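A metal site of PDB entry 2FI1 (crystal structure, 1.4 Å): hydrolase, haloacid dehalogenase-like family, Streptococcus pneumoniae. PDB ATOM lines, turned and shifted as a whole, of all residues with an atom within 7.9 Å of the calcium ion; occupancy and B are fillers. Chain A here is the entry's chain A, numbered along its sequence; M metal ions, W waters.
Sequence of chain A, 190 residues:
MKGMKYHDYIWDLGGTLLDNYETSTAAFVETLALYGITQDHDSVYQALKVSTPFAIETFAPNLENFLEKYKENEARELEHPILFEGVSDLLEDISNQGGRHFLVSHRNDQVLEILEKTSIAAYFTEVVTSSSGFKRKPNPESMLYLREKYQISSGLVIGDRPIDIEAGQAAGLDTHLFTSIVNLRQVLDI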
ATOM      1  N   TRP A  11      -4.199   1.819 -32.390  1.00  0.00           N
ATOM      2  CA  TRP A  11      -4.122   1.003 -31.195  1.00  0.00           C
ATOM      3  C   TRP A  11      -2.938   0.062 -31.184  1.00  0.00           C
ATOM      4  O   TRP A  11      -2.403  -0.323 -32.223  1.00  0.00           O
ATOM      5  CB  TRP A  11      -5.376   0.137 -31.080  1.00  0.00           C
ATOM      6  CG  TRP A  11      -6.670   0.900 -30.932  1.00  0.00           C
ATOM      7  CD1 TRP A  11      -7.537   1.244 -31.926  1.00  0.00           C
ATOM      8  CD2 TRP A  11      -7.244   1.369 -29.705  1.00  0.00           C
ATOM      9  NE1 TRP A  11      -8.607   1.907 -31.396  1.00  0.00           N
ATOM     10  CE2 TRP A  11      -8.452   2.001 -30.048  1.00  0.00           C
ATOM     11  CE3 TRP A  11      -6.855   1.311 -28.361  1.00  0.00           C
ATOM     12  CZ2 TRP A  11      -9.295   2.571 -29.077  1.00  0.00           C
ATOM     13  CZ3 TRP A  11      -7.685   1.889 -27.414  1.00  0.00           C
ATOM     14  CH2 TRP A  11      -8.895   2.511 -27.786  1.00  0.00           C
ATOM     15  N   ASP A  12      -2.585  -0.287 -29.968  1.00  0.00           N
ATOM     16  CA  ASP A  12      -1.662  -1.340 -29.595  1.00  0.00           C
ATOM     17  C   ASP A  12      -2.515  -2.513 -29.106  1.00  0.00           C
ATOM     18  O   ASP A  12      -3.588  -2.314 -28.542  1.00  0.00           O
ATOM     19  CB  ASP A  12      -0.769  -0.744 -28.494  1.00  0.00           C
ATOM     20  CG  ASP A  12       0.058  -1.754 -27.728  1.00  0.00           C
ATOM     21  OD1 ASP A  12       0.797  -2.538 -28.346  1.00  0.00           O
ATOM     22  OD2 ASP A  12       0.022  -1.650 -26.474  1.00  0.00           O
ATOM     23  N   LEU A  13      -2.062  -3.747 -29.328  1.00  0.00           N
ATOM     24  CA  LEU A  13      -2.831  -4.924 -28.948  1.00  0.00           C
ATOM     25  C   LEU A  13      -2.484  -5.341 -27.513  1.00  0.00           C
ATOM     26  O   LEU A  13      -3.211  -5.024 -26.595  1.00  0.00           O
ATOM     27  CB  LEU A  13      -2.596  -6.069 -29.951  1.00  0.00           C
ATOM     28  CG  LEU A  13      -3.406  -7.342 -29.719  1.00  0.00           C
ATOM     29  CD1 LEU A  13      -4.910  -7.071 -29.797  1.00  0.00           C
ATOM     30  CD2 LEU A  13      -3.000  -8.406 -30.730  1.00  0.00           C
ATOM     31  N   GLY A  14      -1.351  -6.006 -27.322  1.00  0.00           N
ATOM     32  CA  GLY A  14      -0.980  -6.499 -26.006  1.00  0.00           C
ATOM     33  C   GLY A  14      -0.824  -5.385 -25.001  1.00  0.00           C
ATOM     34  O   GLY A  14      -0.105  -4.413 -25.260  1.00  0.00           O
ATOM     35  N   GLY A  15      -1.485  -5.502 -23.859  1.00  0.00           N
ATOM     36  CA  GLY A  15      -1.380  -4.515 -22.788  1.00  0.00           C
ATOM     37  C   GLY A  15      -2.286  -3.300 -22.923  1.00  0.00           C
ATOM     38  O   GLY A  15      -2.328  -2.459 -22.017  1.00  0.00           O
ATOM     39  N   THR A  16      -3.022  -3.207 -24.035  1.00  0.00           N
ATOM     40  CA  THR A  16      -3.915  -2.078 -24.288  1.00  0.00           C
ATOM     41  C   THR A  16      -5.312  -2.609 -24.602  1.00  0.00           C
ATOM     42  O   THR A  16      -6.247  -2.374 -23.840  1.00  0.00           O
ATOM     43  CB  THR A  16      -3.357  -1.200 -25.418  1.00  0.00           C
ATOM     44  OG1 THR A  16      -2.090  -0.666 -25.001  1.00  0.00           O
ATOM     45  CG2 THR A  16      -4.290  -0.078 -25.741  1.00  0.00           C
ATOM     46  N   LEU A  17      -5.471  -3.342 -25.704  1.00  0.00           N
ATOM     47  CA  LEU A  17      -6.755  -3.988 -26.003  1.00  0.00           C
ATOM     48  C   LEU A  17      -6.820  -5.407 -25.437  1.00  0.00           C
ATOM     49  O   LEU A  17      -7.848  -5.832 -24.925  1.00  0.00           O
ATOM     50  CB  LEU A  17      -6.985  -4.026 -27.506  1.00  0.00           C
ATOM     51  CG  LEU A  17      -7.113  -2.652 -28.169  1.00  0.00           C
ATOM     52  CD1 LEU A  17      -7.288  -2.867 -29.640  1.00  0.00           C
ATOM     53  CD2 LEU A  17      -8.272  -1.857 -27.598  1.00  0.00           C
ATOM     54  N   LEU A  18      -5.717  -6.139 -25.574  1.00  0.00           N
ATOM     55  CA  LEU A  18      -5.631  -7.533 -25.165  1.00  0.00           C
ATOM     56  C   LEU A  18      -4.899  -7.639 -23.832  1.00  0.00           C
ATOM     57  O   LEU A  18      -3.779  -7.153 -23.711  1.00  0.00           O
ATOM     58  CB  LEU A  18      -4.870  -8.338 -26.219  1.00  0.00           C
ATOM     59  CG  LEU A  18      -4.706  -9.827 -25.960  1.00  0.00           C
ATOM     60  CD1 LEU A  18      -6.027 -10.550 -26.162  1.00  0.00           C
ATOM     61  CD2 LEU A  18      -3.616 -10.375 -26.857  1.00  0.00           C
ATOM     62  N   ASN A  20      -3.010  -9.779 -22.384  1.00  0.00           N
ATOM     63  CA  ASN A  20      -2.190 -10.970 -22.558  1.00  0.00           C
ATOM     64  C   ASN A  20      -1.588 -11.431 -21.239  1.00  0.00           C
ATOM     65  O   ASN A  20      -1.337 -12.627 -21.063  1.00  0.00           O
ATOM     66  CB  ASN A  20      -1.082 -10.749 -23.596  1.00  0.00           C
ATOM     67  CG  ASN A  20      -0.193  -9.588 -23.250  1.00  0.00           C
ATOM     68  OD1 ASN A  20      -0.557  -8.434 -23.484  1.00  0.00           O
ATOM     69  ND2 ASN A  20       0.989  -9.863 -22.696  1.00  0.00           N
ATOM     70  N   TYR A  21      -1.334 -10.516 -20.301  1.00  0.00           N
ATOM     71  CA  TYR A  21      -0.753 -10.952 -19.032  1.00  0.00           C
ATOM     72  C   TYR A  21      -1.748 -11.759 -18.222  1.00  0.00           C
ATOM     73  O   TYR A  21      -1.334 -12.566 -17.387  1.00  0.00           O
ATOM     74  CB  TYR A  21      -0.132  -9.783 -18.263  1.00  0.00           C
ATOM     75  CG  TYR A  21       1.097  -9.249 -18.971  1.00  0.00           C
ATOM     76  CD1 TYR A  21       2.223 -10.054 -19.129  1.00  0.00           C
ATOM     77  CD2 TYR A  21       1.123  -7.972 -19.495  1.00  0.00           C
ATOM     78  CE1 TYR A  21       3.344  -9.577 -19.809  1.00  0.00           C
ATOM     79  CE2 TYR A  21       2.249  -7.490 -20.162  1.00  0.00           C
ATOM     80  CZ  TYR A  21       3.346  -8.304 -20.313  1.00  0.00           C
ATOM     81  OH  TYR A  21       4.455  -7.835 -20.968  1.00  0.00           O
ATOM     82  N   VAL A 104      -1.427  -1.398 -34.900  1.00  0.00           N
ATOM     83  CA  VAL A 104      -0.037  -1.647 -35.274  1.00  0.00           C
ATOM     84  C   VAL A 104       0.554  -2.645 -34.297  1.00  0.00           C
ATOM     85  O   VAL A 104       0.529  -2.422 -33.073  1.00  0.00           O
ATOM     86  CB  VAL A 104       0.798  -0.357 -35.294  1.00  0.00           C
ATOM     87  CG1 VAL A 104       2.276  -0.668 -35.534  1.00  0.00           C
ATOM     88  CG2 VAL A 104       0.297   0.575 -36.364  1.00  0.00           C
ATOM     89  N   LYS A 137       8.327  -0.026 -33.592  1.00  0.00           N
ATOM     90  CA  LYS A 137       8.248   1.107 -32.683  1.00  0.00           C
ATOM     91  C   LYS A 137       9.495   1.047 -31.777  1.00  0.00           C
ATOM     92  O   LYS A 137       9.922  -0.038 -31.393  1.00  0.00           O
ATOM     93  CB  LYS A 137       6.955   1.042 -31.860  1.00  0.00           C
ATOM     94  CG  LYS A 137       5.685   1.086 -32.717  1.00  0.00           C
ATOM     95  CD  LYS A 137       4.418   0.878 -31.904  1.00  0.00           C
ATOM     96  CE  LYS A 137       4.232  -0.573 -31.471  1.00  0.00           C
ATOM     97  NZ  LYS A 137       3.013  -0.761 -30.621  1.00  0.00           N
ATOM     98  N   ILE A 158      -2.633   5.076 -29.026  1.00  0.00           N
ATOM     99  CA  ILE A 158      -2.864   4.538 -27.698  1.00  0.00           C
ATOM    100  C   ILE A 158      -2.008   3.285 -27.502  1.00  0.00           C
ATOM    101  O   ILE A 158      -2.115   2.337 -28.268  1.00  0.00           O
ATOM    102  CB  ILE A 158      -4.340   4.154 -27.480  1.00  0.00           C
ATOM    103  CG1 ILE A 158      -5.266   5.333 -27.814  1.00  0.00           C
ATOM    104  CG2 ILE A 158      -4.549   3.700 -26.049  1.00  0.00           C
ATOM    105  CD1 ILE A 158      -5.860   5.250 -29.202  1.00  0.00           C
ATOM    106  N   GLY A 159      -1.159   3.288 -26.485  1.00  0.00           N
ATOM    107  CA  GLY A 159      -0.355   2.111 -26.183  1.00  0.00           C
ATOM    108  C   GLY A 159       0.109   2.142 -24.743  1.00  0.00           C
ATOM    109  O   GLY A 159       0.061   3.189 -24.091  1.00  0.00           O
ATOM    110  N   ASP A 160       0.569   1.008 -24.254  1.00  0.00           N
ATOM    111  CA  ASP A 160       0.933   0.904 -22.840  1.00  0.00           C
ATOM    112  C   ASP A 160       2.408   1.138 -22.561  1.00  0.00           C
ATOM    113  O   ASP A 160       2.792   1.208 -21.390  1.00  0.00           O
ATOM    114  CB  ASP A 160       0.506  -0.452 -22.260  1.00  0.00           C
ATOM    115  CG  ASP A 160       1.253  -1.637 -22.841  1.00  0.00           C
ATOM    116  OD1 ASP A 160       1.557  -1.631 -24.057  1.00  0.00           O
ATOM    117  OD2 ASP A 160       1.544  -2.596 -22.090  1.00  0.00           O
ATOM    118  N   ARG A 161       3.237   1.265 -23.589  1.00  0.00           N
ATOM    119  CA  ARG A 161       4.684   1.365 -23.400  1.00  0.00           C
ATOM    120  C   ARG A 161       5.277   2.666 -23.921  1.00  0.00           C
ATOM    121  O   ARG A 161       4.761   3.272 -24.860  1.00  0.00           O
ATOM    122  CB  ARG A 161       5.383   0.193 -24.098  1.00  0.00           C
ATOM    123  CG  ARG A 161       5.212  -1.128 -23.428  1.00  0.00           C
ATOM    124  CD  ARG A 161       5.943  -2.217 -24.181  1.00  0.00           C
ATOM    125  NE  ARG A 161       7.372  -1.920 -24.327  1.00  0.00           N
ATOM    126  CZ  ARG A 161       8.196  -2.576 -25.132  1.00  0.00           C
ATOM    127  NH1 ARG A 161       7.752  -3.583 -25.871  1.00  0.00           N
ATOM    128  NH2 ARG A 161       9.474  -2.240 -25.198  1.00  0.00           N
ATOM    129  N   ILE A 163       7.653   3.068 -25.974  1.00  0.00           N
ATOM    130  CA  ILE A 163       7.916   3.043 -27.414  1.00  0.00           C
ATOM    131  C   ILE A 163       6.680   3.392 -28.253  1.00  0.00           C
ATOM    132  O   ILE A 163       6.802   3.898 -29.374  1.00  0.00           O
ATOM    133  CB  ILE A 163       8.511   1.700 -27.915  1.00  0.00           C
ATOM    134  CG1 ILE A 163       7.577   0.522 -27.644  1.00  0.00           C
ATOM    135  CG2 ILE A 163       9.902   1.494 -27.306  1.00  0.00           C
ATOM    136  CD1 ILE A 163       8.011  -0.761 -28.323  1.00  0.00           C
ATOM    137  N   ASP A 164       5.491   3.152 -27.691  1.00  0.00           N
ATOM    138  CA  ASP A 164       4.250   3.497 -28.387  1.00  0.00           C
ATOM    139  C   ASP A 164       4.069   4.999 -28.431  1.00  0.00           C
ATOM    140  O   ASP A 164       3.720   5.579 -29.463  1.00  0.00           O
ATOM    141  CB  ASP A 164       3.065   2.843 -27.673  1.00  0.00           C
ATOM    142  CG  ASP A 164       3.203   1.338 -27.578  1.00  0.00           C
ATOM    143  OD1 ASP A 164       3.729   0.698 -28.525  1.00  0.00           O
ATOM    144  OD2 ASP A 164       2.862   0.807 -26.510  1.00  0.00           O
HETATM  145 CA    CA M   1       1.736  -3.174 -25.826  1.00  0.00          CA
HETATM  146  O   HOH W   1       2.708  -4.315 -23.960  1.00  0.00           O
HETATM  147  O   HOH W   2       2.468  -4.884 -27.229  1.00  0.00           O
HETATM  148  O   HOH W   3       3.529  -1.789 -26.563  1.00  0.00           O
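O of Gly 14 binds the calcium ion (2.3 Å). The calcium ion is bound by water W2 (2.3 Å). The calcium ion is bound by the side-chain carboxylate (OD1) of Asp 160 (2.4 Å). The calcium ion is bound by water W3, at 2.4 Å. OD2 of Asp 12 binds the calcium ion, 2.4 Å away. Water W1 is bound to the calcium ion, at 2.4 Å. OD1 of Asp 12 is bound to the calcium ion (2.8 Å).
The nearest printed residue that does not touch the calcium ion is Asp 164 (4.2 Å).
N of Asp 160 lies within hydrogen-bond range of OD2 of Asp 164 (3.2 Å). The backbone NH of Asp 160 is in hydrogen-bond range of the side-chain hydroxyl of Thr 16, 3.2 Å away. N of Asp 12 lies within hydrogen-bond range of O of Ile 158, at 3.2 Å. OG1 of Thr 16 lies close to OD2 of Asp 12 (2.8 Å). The side-chain amino group (NZ) of Lys 137 sits close to the side-chain carboxylate (OD1) of Asp 12 (3.6 Å).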
